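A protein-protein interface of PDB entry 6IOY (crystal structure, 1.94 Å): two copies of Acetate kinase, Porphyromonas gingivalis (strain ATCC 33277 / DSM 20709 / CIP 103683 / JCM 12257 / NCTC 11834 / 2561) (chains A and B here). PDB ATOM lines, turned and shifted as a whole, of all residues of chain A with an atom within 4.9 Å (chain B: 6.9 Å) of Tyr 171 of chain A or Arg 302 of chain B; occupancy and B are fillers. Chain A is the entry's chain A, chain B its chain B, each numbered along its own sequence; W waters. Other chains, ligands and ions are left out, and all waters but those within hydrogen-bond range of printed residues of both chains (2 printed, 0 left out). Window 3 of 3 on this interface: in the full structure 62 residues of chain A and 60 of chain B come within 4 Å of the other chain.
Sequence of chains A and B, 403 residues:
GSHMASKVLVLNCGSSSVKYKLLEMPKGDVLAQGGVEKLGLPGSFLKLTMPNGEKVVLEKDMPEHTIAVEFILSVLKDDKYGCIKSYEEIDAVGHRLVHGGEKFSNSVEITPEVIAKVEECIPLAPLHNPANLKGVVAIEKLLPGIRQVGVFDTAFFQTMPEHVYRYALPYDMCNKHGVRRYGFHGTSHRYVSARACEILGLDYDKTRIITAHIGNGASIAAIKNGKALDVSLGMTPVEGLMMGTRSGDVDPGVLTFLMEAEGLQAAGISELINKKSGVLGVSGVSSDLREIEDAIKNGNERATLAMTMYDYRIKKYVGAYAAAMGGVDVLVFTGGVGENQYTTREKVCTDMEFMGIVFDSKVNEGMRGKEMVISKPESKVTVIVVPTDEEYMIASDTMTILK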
ATOM      1  N   GLU A 162      -3.418 -13.303 -10.678  1.00  0.00           N
ATOM      2  CA  GLU A 162      -3.430 -12.437  -9.488  1.00  0.00           C
ATOM      3  C   GLU A 162      -3.687 -10.969  -9.862  1.00  0.00           C
ATOM      4  O   GLU A 162      -4.329 -10.263  -9.101  1.00  0.00           O
ATOM      5  CB  GLU A 162      -2.114 -12.574  -8.728  1.00  0.00           C
ATOM      6  CG  GLU A 162      -2.105 -11.802  -7.419  1.00  0.00           C
ATOM      7  CD  GLU A 162      -0.886 -12.077  -6.554  1.00  0.00           C
ATOM      8  OE1 GLU A 162       0.065 -12.719  -7.041  1.00  0.00           O
ATOM      9  OE2 GLU A 162      -0.854 -11.561  -5.422  1.00  0.00           O
ATOM     10  N   ARG A 166      -6.740  -9.906  -7.363  1.00  0.00           N
ATOM     11  CA  ARG A 166      -6.359  -9.060  -6.222  1.00  0.00           C
ATOM     12  C   ARG A 166      -7.045  -7.698  -6.359  1.00  0.00           C
ATOM     13  O   ARG A 166      -7.141  -7.154  -7.470  1.00  0.00           O
ATOM     14  CB  ARG A 166      -4.832  -8.908  -6.149  1.00  0.00           C
ATOM     15  CG  ARG A 166      -4.335  -8.092  -4.971  1.00  0.00           C
ATOM     16  CD  ARG A 166      -2.869  -8.211  -4.666  1.00  0.00           C
ATOM     17  NE  ARG A 166      -2.531  -9.540  -4.180  1.00  0.00           N
ATOM     18  CZ  ARG A 166      -2.724  -9.978  -2.939  1.00  0.00           C
ATOM     19  NH1 ARG A 166      -3.345  -9.206  -2.048  1.00  0.00           N
ATOM     20  NH2 ARG A 166      -2.300 -11.179  -2.595  1.00  0.00           N
ATOM     21  N   LEU A 169      -6.114  -3.007  -2.485  1.00  0.00           N
ATOM     22  CA  LEU A 169      -6.326  -2.722  -1.068  1.00  0.00           C
ATOM     23  C   LEU A 169      -5.057  -3.121  -0.314  1.00  0.00           C
ATOM     24  O   LEU A 169      -4.175  -3.758  -0.896  1.00  0.00           O
ATOM     25  CB  LEU A 169      -7.545  -3.526  -0.604  1.00  0.00           C
ATOM     26  CG  LEU A 169      -8.900  -3.043  -1.133  1.00  0.00           C
ATOM     27  CD1 LEU A 169      -9.994  -4.002  -0.760  1.00  0.00           C
ATOM     28  CD2 LEU A 169      -9.258  -1.662  -0.631  1.00  0.00           C
ATOM     29  N   PRO A 170      -4.917  -2.793   0.990  1.00  0.00           N
ATOM     30  CA  PRO A 170      -3.715  -3.161   1.734  1.00  0.00           C
ATOM     31  C   PRO A 170      -3.414  -4.668   1.635  1.00  0.00           C
ATOM     32  O   PRO A 170      -4.248  -5.521   1.941  1.00  0.00           O
ATOM     33  CB  PRO A 170      -4.004  -2.722   3.182  1.00  0.00           C
ATOM     34  CG  PRO A 170      -5.101  -1.672   3.050  1.00  0.00           C
ATOM     35  CD  PRO A 170      -5.891  -2.071   1.813  1.00  0.00           C
ATOM     36  N   TYR A 171      -2.202  -4.970   1.178  1.00  0.00           N
ATOM     37  CA  TYR A 171      -1.777  -6.289   0.780  1.00  0.00           C
ATOM     38  C   TYR A 171      -1.907  -7.281   1.933  1.00  0.00           C
ATOM     39  O   TYR A 171      -2.557  -8.317   1.794  1.00  0.00           O
ATOM     40  CB  TYR A 171      -0.348  -6.199   0.258  1.00  0.00           C
ATOM     41  CG  TYR A 171       0.231  -7.458  -0.330  1.00  0.00           C
ATOM     42  CD1 TYR A 171      -0.043  -7.834  -1.645  1.00  0.00           C
ATOM     43  CD2 TYR A 171       1.122  -8.238   0.394  1.00  0.00           C
ATOM     44  CE1 TYR A 171       0.552  -8.952  -2.205  1.00  0.00           C
ATOM     45  CE2 TYR A 171       1.722  -9.359  -0.162  1.00  0.00           C
ATOM     46  CZ  TYR A 171       1.423  -9.723  -1.465  1.00  0.00           C
ATOM     47  OH  TYR A 171       1.957 -10.836  -2.058  1.00  0.00           O
ATOM     48  N   ASP A 172      -1.295  -6.949   3.068  1.00  0.00           N
ATOM     49  CA  ASP A 172      -1.279  -7.869   4.233  1.00  0.00           C
ATOM     50  C   ASP A 172      -2.699  -8.107   4.739  1.00  0.00           C
ATOM     51  O   ASP A 172      -3.031  -9.226   5.053  1.00  0.00           O
ATOM     52  CB  ASP A 172      -0.384  -7.375   5.373  1.00  0.00           C
ATOM     53  CG  ASP A 172       1.109  -7.533   5.146  1.00  0.00           C
ATOM     54  OD1 ASP A 172       1.501  -8.251   4.170  1.00  0.00           O
ATOM     55  OD2 ASP A 172       1.868  -6.989   5.941  1.00  0.00           O
ATOM     56  N   MET A 173      -3.529  -7.057   4.784  1.00  0.00           N
ATOM     57  CA  MET A 173      -4.888  -7.190   5.292  1.00  0.00           C
ATOM     58  C   MET A 173      -5.721  -8.106   4.385  1.00  0.00           C
ATOM     59  O   MET A 173      -6.439  -8.994   4.879  1.00  0.00           O
ATOM     60  CB  MET A 173      -5.550  -5.821   5.405  1.00  0.00           C
ATOM     61  CG  MET A 173      -6.948  -5.873   5.989  1.00  0.00           C
ATOM     62  SD  MET A 173      -7.599  -4.164   6.154  1.00  0.00           S
ATOM     63  CE  MET A 173      -6.608  -3.559   7.527  1.00  0.00           C
ATOM     64  N   CYS A 174      -5.588  -7.945   3.061  1.00  0.00           N
ATOM     65  CA  CYS A 174      -6.261  -8.831   2.139  1.00  0.00           C
ATOM     66  C   CYS A 174      -5.815 -10.288   2.339  1.00  0.00           C
ATOM     67  O   CYS A 174      -6.637 -11.185   2.418  1.00  0.00           O
ATOM     68  CB  CYS A 174      -6.030  -8.376   0.700  1.00  0.00           C
ATOM     69  SG  CYS A 174      -7.021  -6.884   0.359  1.00  0.00           S
ATOM     70  N   ASN A 175      -4.504 -10.506   2.447  1.00  0.00           N
ATOM     71  CA  ASN A 175      -3.973 -11.863   2.541  1.00  0.00           C
ATOM     72  C   ASN A 175      -4.428 -12.497   3.858  1.00  0.00           C
ATOM     73  O   ASN A 175      -4.785 -13.663   3.893  1.00  0.00           O
ATOM     74  CB  ASN A 175      -2.459 -11.886   2.393  1.00  0.00           C
ATOM     75  CG  ASN A 175      -1.991 -11.462   1.012  1.00  0.00           C
ATOM     76  OD1 ASN A 175      -2.745 -11.563   0.041  1.00  0.00           O
ATOM     77  ND2 ASN A 175      -0.749 -11.018   0.911  1.00  0.00           N
ATOM     78  N   LYS B 276      -3.986   4.058   2.053  1.00  0.00           N
ATOM     79  CA  LYS B 276      -3.183   2.861   2.260  1.00  0.00           C
ATOM     80  C   LYS B 276      -3.340   1.870   1.107  1.00  0.00           C
ATOM     81  O   LYS B 276      -2.815   0.760   1.180  1.00  0.00           O
ATOM     82  CB  LYS B 276      -3.587   2.232   3.594  1.00  0.00           C
ATOM     83  CG  LYS B 276      -3.114   3.020   4.818  1.00  0.00           C
ATOM     84  CD  LYS B 276      -1.651   3.452   4.712  1.00  0.00           C
ATOM     85  CE  LYS B 276      -1.000   3.835   6.022  1.00  0.00           C
ATOM     86  NZ  LYS B 276      -1.757   4.916   6.685  1.00  0.00           N
ATOM     87  N   VAL B 279      -1.446   1.767  -5.690  1.00  0.00           N
ATOM     88  CA  VAL B 279      -0.092   1.339  -6.012  1.00  0.00           C
ATOM     89  C   VAL B 279       0.722   1.167  -4.721  1.00  0.00           C
ATOM     90  O   VAL B 279       1.499   0.227  -4.610  1.00  0.00           O
ATOM     91  CB  VAL B 279       0.551   2.343  -6.979  1.00  0.00           C
ATOM     92  CG1 VAL B 279       2.046   2.156  -7.109  1.00  0.00           C
ATOM     93  CG2 VAL B 279      -0.147   2.285  -8.342  1.00  0.00           C
ATOM     94  N   LEU B 280       0.542   2.081  -3.770  1.00  0.00           N
ATOM     95  CA  LEU B 280       1.288   2.052  -2.490  1.00  0.00           C
ATOM     96  C   LEU B 280       0.930   0.770  -1.736  1.00  0.00           C
ATOM     97  O   LEU B 280       1.828   0.020  -1.316  1.00  0.00           O
ATOM     98  CB  LEU B 280       0.971   3.298  -1.660  1.00  0.00           C
ATOM     99  CG  LEU B 280       1.493   3.236  -0.217  1.00  0.00           C
ATOM    100  CD1 LEU B 280       2.996   3.105  -0.188  1.00  0.00           C
ATOM    101  CD2 LEU B 280       1.075   4.436   0.616  1.00  0.00           C
ATOM    102  N   GLY B 281      -0.376   0.534  -1.576  1.00  0.00           N
ATOM    103  CA  GLY B 281      -0.899  -0.596  -0.854  1.00  0.00           C
ATOM    104  C   GLY B 281      -0.488  -1.939  -1.435  1.00  0.00           C
ATOM    105  O   GLY B 281      -0.112  -2.833  -0.674  1.00  0.00           O
ATOM    106  N   VAL B 282      -0.515  -2.081  -2.767  1.00  0.00           N
ATOM    107  CA  VAL B 282      -0.147  -3.365  -3.379  1.00  0.00           C
ATOM    108  C   VAL B 282       1.385  -3.527  -3.405  1.00  0.00           C
ATOM    109  O   VAL B 282       1.905  -4.603  -2.997  1.00  0.00           O
ATOM    110  CB  VAL B 282      -0.729  -3.526  -4.795  1.00  0.00           C
ATOM    111  CG1 VAL B 282      -0.238  -4.809  -5.439  1.00  0.00           C
ATOM    112  CG2 VAL B 282      -2.253  -3.506  -4.781  1.00  0.00           C
ATOM    113  N   SER B 283       2.093  -2.496  -3.894  1.00  0.00           N
ATOM    114  CA  SER B 283       3.552  -2.541  -4.102  1.00  0.00           C
ATOM    115  C   SER B 283       4.303  -2.743  -2.777  1.00  0.00           C
ATOM    116  O   SER B 283       5.282  -3.489  -2.741  1.00  0.00           O
ATOM    117  CB  SER B 283       4.066  -1.323  -4.830  1.00  0.00           C
ATOM    118  OG  SER B 283       4.088  -0.183  -3.993  1.00  0.00           O
ATOM    119  N   GLY B 284       3.835  -2.080  -1.722  1.00  0.00           N
ATOM    120  CA  GLY B 284       4.596  -1.964  -0.480  1.00  0.00           C
ATOM    121  C   GLY B 284       5.869  -1.153  -0.654  1.00  0.00           C
ATOM    122  O   GLY B 284       6.798  -1.238   0.167  1.00  0.00           O
ATOM    123  N   VAL B 285       5.918  -0.348  -1.719  1.00  0.00           N
ATOM    124  CA  VAL B 285       7.103   0.405  -2.074  1.00  0.00           C
ATOM    125  C   VAL B 285       6.770   1.892  -1.942  1.00  0.00           C
ATOM    126  O   VAL B 285       7.276   2.554  -1.068  1.00  0.00           O
ATOM    127  CB  VAL B 285       7.600   0.047  -3.483  1.00  0.00           C
ATOM    128  CG1 VAL B 285       8.746   0.939  -3.924  1.00  0.00           C
ATOM    129  CG2 VAL B 285       8.017  -1.412  -3.555  1.00  0.00           C
ATOM    130  N   ILE B 292       8.413   2.896  -8.211  1.00  0.00           N
ATOM    131  CA  ILE B 292       7.920   1.566  -8.605  1.00  0.00           C
ATOM    132  C   ILE B 292       8.822   1.022  -9.711  1.00  0.00           C
ATOM    133  O   ILE B 292       9.301  -0.111  -9.612  1.00  0.00           O
ATOM    134  CB  ILE B 292       6.442   1.585  -9.046  1.00  0.00           C
ATOM    135  CG1 ILE B 292       5.508   2.043  -7.925  1.00  0.00           C
ATOM    136  CG2 ILE B 292       6.026   0.219  -9.573  1.00  0.00           C
ATOM    137  CD1 ILE B 292       5.585   1.194  -6.705  1.00  0.00           C
ATOM    138  N   ILE B 296      10.998  -2.371  -9.752  1.00  0.00           N
ATOM    139  CA  ILE B 296      10.768  -3.415 -10.747  1.00  0.00           C
ATOM    140  C   ILE B 296      12.112  -3.867 -11.338  1.00  0.00           C
ATOM    141  O   ILE B 296      12.314  -5.085 -11.488  1.00  0.00           O
ATOM    142  CB  ILE B 296       9.764  -2.982 -11.841  1.00  0.00           C
ATOM    143  CG1 ILE B 296       8.339  -2.913 -11.283  1.00  0.00           C
ATOM    144  CG2 ILE B 296       9.842  -3.915 -13.043  1.00  0.00           C
ATOM    145  CD1 ILE B 296       7.321  -2.275 -12.195  1.00  0.00           C
ATOM    146  N   GLY B 299      13.829  -6.288  -9.442  1.00  0.00           N
ATOM    147  CA  GLY B 299      13.027  -7.539  -9.378  1.00  0.00           C
ATOM    148  C   GLY B 299      12.100  -7.627  -8.170  1.00  0.00           C
ATOM    149  O   GLY B 299      11.886  -8.710  -7.629  1.00  0.00           O
ATOM    150  N   ASN B 300      11.519  -6.494  -7.756  1.00  0.00           N
ATOM    151  CA  ASN B 300      10.470  -6.487  -6.712  1.00  0.00           C
ATOM    152  C   ASN B 300       9.166  -6.975  -7.364  1.00  0.00           C
ATOM    153  O   ASN B 300       8.610  -6.268  -8.206  1.00  0.00           O
ATOM    154  CB  ASN B 300      10.314  -5.113  -6.061  1.00  0.00           C
ATOM    155  CG  ASN B 300       9.276  -5.103  -4.953  1.00  0.00           C
ATOM    156  OD1 ASN B 300       8.218  -5.754  -5.016  1.00  0.00           O
ATOM    157  ND2 ASN B 300       9.540  -4.340  -3.922  1.00  0.00           N
ATOM    158  N   GLU B 301       8.695  -8.157  -6.957  1.00  0.00           N
ATOM    159  CA  GLU B 301       7.555  -8.811  -7.592  1.00  0.00           C
ATOM    160  C   GLU B 301       6.236  -8.095  -7.256  1.00  0.00           C
ATOM    161  O   GLU B 301       5.362  -8.024  -8.105  1.00  0.00           O
ATOM    162  CB  GLU B 301       7.507 -10.292  -7.223  1.00  0.00           C
ATOM    163  CG  GLU B 301       8.598 -11.102  -7.901  1.00  0.00           C
ATOM    164  CD  GLU B 301       8.606 -11.081  -9.425  1.00  0.00           C
ATOM    165  OE1 GLU B 301       7.604 -10.687 -10.060  1.00  0.00           O
ATOM    166  OE2 GLU B 301       9.653 -11.479  -9.973  1.00  0.00           O
ATOM    167  N   ARG B 302       6.109  -7.567  -6.037  1.00  0.00           N
ATOM    168  CA  ARG B 302       4.913  -6.843  -5.626  1.00  0.00           C
ATOM    169  C   ARG B 302       4.787  -5.539  -6.445  1.00  0.00           C
ATOM    170  O   ARG B 302       3.644  -5.120  -6.761  1.00  0.00           O
ATOM    171  CB  ARG B 302       4.943  -6.581  -4.129  1.00  0.00           C
ATOM    172  CG  ARG B 302       4.303  -7.680  -3.307  1.00  0.00           C
ATOM    173  CD  ARG B 302       4.325  -7.414  -1.818  1.00  0.00           C
ATOM    174  NE  ARG B 302       3.569  -6.223  -1.457  1.00  0.00           N
ATOM    175  CZ  ARG B 302       3.494  -5.748  -0.235  1.00  0.00           C
ATOM    176  NH1 ARG B 302       4.218  -6.289   0.730  1.00  0.00           N
ATOM    177  NH2 ARG B 302       2.693  -4.724   0.032  1.00  0.00           N
ATOM    178  N   ALA B 303       5.906  -4.873  -6.744  1.00  0.00           N
ATOM    179  CA  ALA B 303       5.912  -3.677  -7.574  1.00  0.00           C
ATOM    180  C   ALA B 303       5.488  -4.012  -8.998  1.00  0.00           C
ATOM    181  O   ALA B 303       4.713  -3.286  -9.589  1.00  0.00           O
ATOM    182  CB  ALA B 303       7.268  -2.993  -7.578  1.00  0.00           C
ATOM    183  N   THR B 304       5.991  -5.115  -9.537  1.00  0.00           N
ATOM    184  CA  THR B 304       5.584  -5.582 -10.857  1.00  0.00           C
ATOM    185  C   THR B 304       4.069  -5.852 -10.863  1.00  0.00           C
ATOM    186  O   THR B 304       3.378  -5.468 -11.817  1.00  0.00           O
ATOM    187  CB  THR B 304       6.362  -6.829 -11.295  1.00  0.00           C
ATOM    188  OG1 THR B 304       7.717  -6.418 -11.444  1.00  0.00           O
ATOM    189  CG2 THR B 304       5.837  -7.429 -12.577  1.00  0.00           C
ATOM    190  N   LEU B 305       3.579  -6.524  -9.822  1.00  0.00           N
ATOM    191  CA  LEU B 305       2.173  -6.864  -9.706  1.00  0.00           C
ATOM    192  C   LEU B 305       1.330  -5.586  -9.687  1.00  0.00           C
ATOM    193  O   LEU B 305       0.288  -5.515 -10.368  1.00  0.00           O
ATOM    194  CB  LEU B 305       1.936  -7.673  -8.435  1.00  0.00           C
ATOM    195  CG  LEU B 305       0.468  -7.896  -8.083  1.00  0.00           C
ATOM    196  CD1 LEU B 305      -0.220  -8.691  -9.163  1.00  0.00           C
ATOM    197  CD2 LEU B 305       0.331  -8.566  -6.745  1.00  0.00           C
ATOM    198  N   ALA B 306       1.757  -4.593  -8.888  1.00  0.00           N
ATOM    199  CA  ALA B 306       1.016  -3.331  -8.782  1.00  0.00           C
ATOM    200  C   ALA B 306       0.807  -2.740 -10.173  1.00  0.00           C
ATOM    201  O   ALA B 306      -0.312  -2.338 -10.518  1.00  0.00           O
ATOM    202  CB  ALA B 306       1.706  -2.335  -7.904  1.00  0.00           C
ATOM    203  N   MET B 307       1.861  -2.746 -10.973  1.00  0.00           N
ATOM    204  CA  MET B 307       1.822  -2.099 -12.298  1.00  0.00           C
ATOM    205  C   MET B 307       0.995  -2.924 -13.286  1.00  0.00           C
ATOM    206  O   MET B 307       0.328  -2.356 -14.139  1.00  0.00           O
ATOM    207  CB  MET B 307       3.244  -1.872 -12.804  1.00  0.00           C
ATOM    208  CG  MET B 307       3.991  -0.808 -12.014  1.00  0.00           C
ATOM    209  SD  MET B 307       2.986   0.732 -11.924  1.00  0.00           S
ATOM    210  CE  MET B 307       2.754   1.069 -13.678  1.00  0.00           C
ATOM    211  N   MET B 309      -1.613  -4.740 -12.471  1.00  0.00           N
ATOM    212  CA  MET B 309      -2.982  -4.433 -12.066  1.00  0.00           C
ATOM    213  C   MET B 309      -3.411  -3.044 -12.582  1.00  0.00           C
ATOM    214  O   MET B 309      -4.535  -2.857 -13.046  1.00  0.00           O
ATOM    215  CB  MET B 309      -3.085  -4.443 -10.537  1.00  0.00           C
ATOM    216  CG  MET B 309      -2.926  -5.816  -9.933  1.00  0.00           C
ATOM    217  SD  MET B 309      -2.870  -5.763  -8.090  1.00  0.00           S
ATOM    218  CE  MET B 309      -4.476  -5.059  -7.727  1.00  0.00           C
HETATM  219  O   HOH W   1      -0.394  -2.763   1.755  1.00  0.00           O
HETATM  220  O   HOH W   2       3.194  -5.750   3.372  1.00  0.00           O
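The side-chain carboxylate (OE2) of Glu 162 of chain A is in salt-bridge range of the guanidinium group (NE) of Arg 166 of chain A, at 2.9 Å. NH2 of Arg 166 of chain A lies within hydrogen-bond range of OD1 of Asn 175 of chain A (2.7 Å). O of Pro 170 of chain A sits at hydrogen-bond distance from SG of Cys 174 of chain A, at 3.5 Å. The backbone carbonyl oxygen (O) of Tyr 171 of chain A sits close to the side-chain amide nitrogen (ND2) of Asn 175 of chain A. The backbone carbonyl oxygen (O) of Gly 281 of chain B lies within hydrogen-bond range of the guanidinium group (NH2) of Arg 302 of chain B, at 3.5 Å. The backbone NH (N) of Arg 302 of chain B is in hydrogen-bond range of the side-chain amide oxygen (OD1) of Asn 300 of chain B (3.0 Å).
Among the printed residues, pairs that only touch across the chains: Glu 162 of chain A with Leu 305 of chain B (3.5 Å), Arg 166 of chain A with Leu 305 of chain B (3.8 Å), Arg 166 of chain A with Met 309 of chain B (3.4 Å), Pro 170 of chain A with Lys 276 of chain B (3.8 Å), Tyr 171 of chain A with Gly 281 of chain B (3.5 Å) and Tyr 171 of chain A with Arg 302 of chain B (3.4 Å).
Printed residues of chain B within 4 Å of Glu 162 of chain A: Leu 305. Of the printed residues of chain B, Arg 166 of chain A touches Leu 305 (3.8 Å) and Met 309 (3.4 Å). Of the printed residues of chain B, Tyr 171 of chain A touches Gly 281 and Arg 302. Printed residues of chain A within 4 Å of Gly 281 of chain B: Tyr 171. Ser 283 of chain B touches none of the printed residues of chain A. Of the printed residues of chain A, Leu 305 of chain B touches Glu 162 (3.5 Å) and Arg 166 (3.8 Å). The nearest printed residue of chain B that does not touch Tyr 171 of chain A is Val 282 of chain B (4.01 Å). The nearest residue of chain A that does not touch Arg 302 of chain B is Asp 172 of chain A (4.8 Å).
Printed residues of chain B that touch a printed residue of chain A: Lys 276, Gly 281, Arg 302, Leu 305 and Met 309. Of the 9 printed residues of chain A, 4 touch a printed residue of chain B. Among the printed residues, 6 pairs touch across the chains. Among the printed residues, no Asp or Glu carboxylate lies within 4 Å of a Lys or Arg side-chain nitrogen of the other chain.
No position is printed for both chains. Of the 6 pairs that touch across the chains among the printed residues, none has its exchanged pair printed and touching as well.
Water W1 lies within hydrogen-bond range of O of Gly 281 of chain B (2.4 Å) and N of Tyr 171 of chain A (2.9 Å). Water W2 bridges NH1 of Arg 302 of chain B and OD1 of Asp 172 of chain A.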
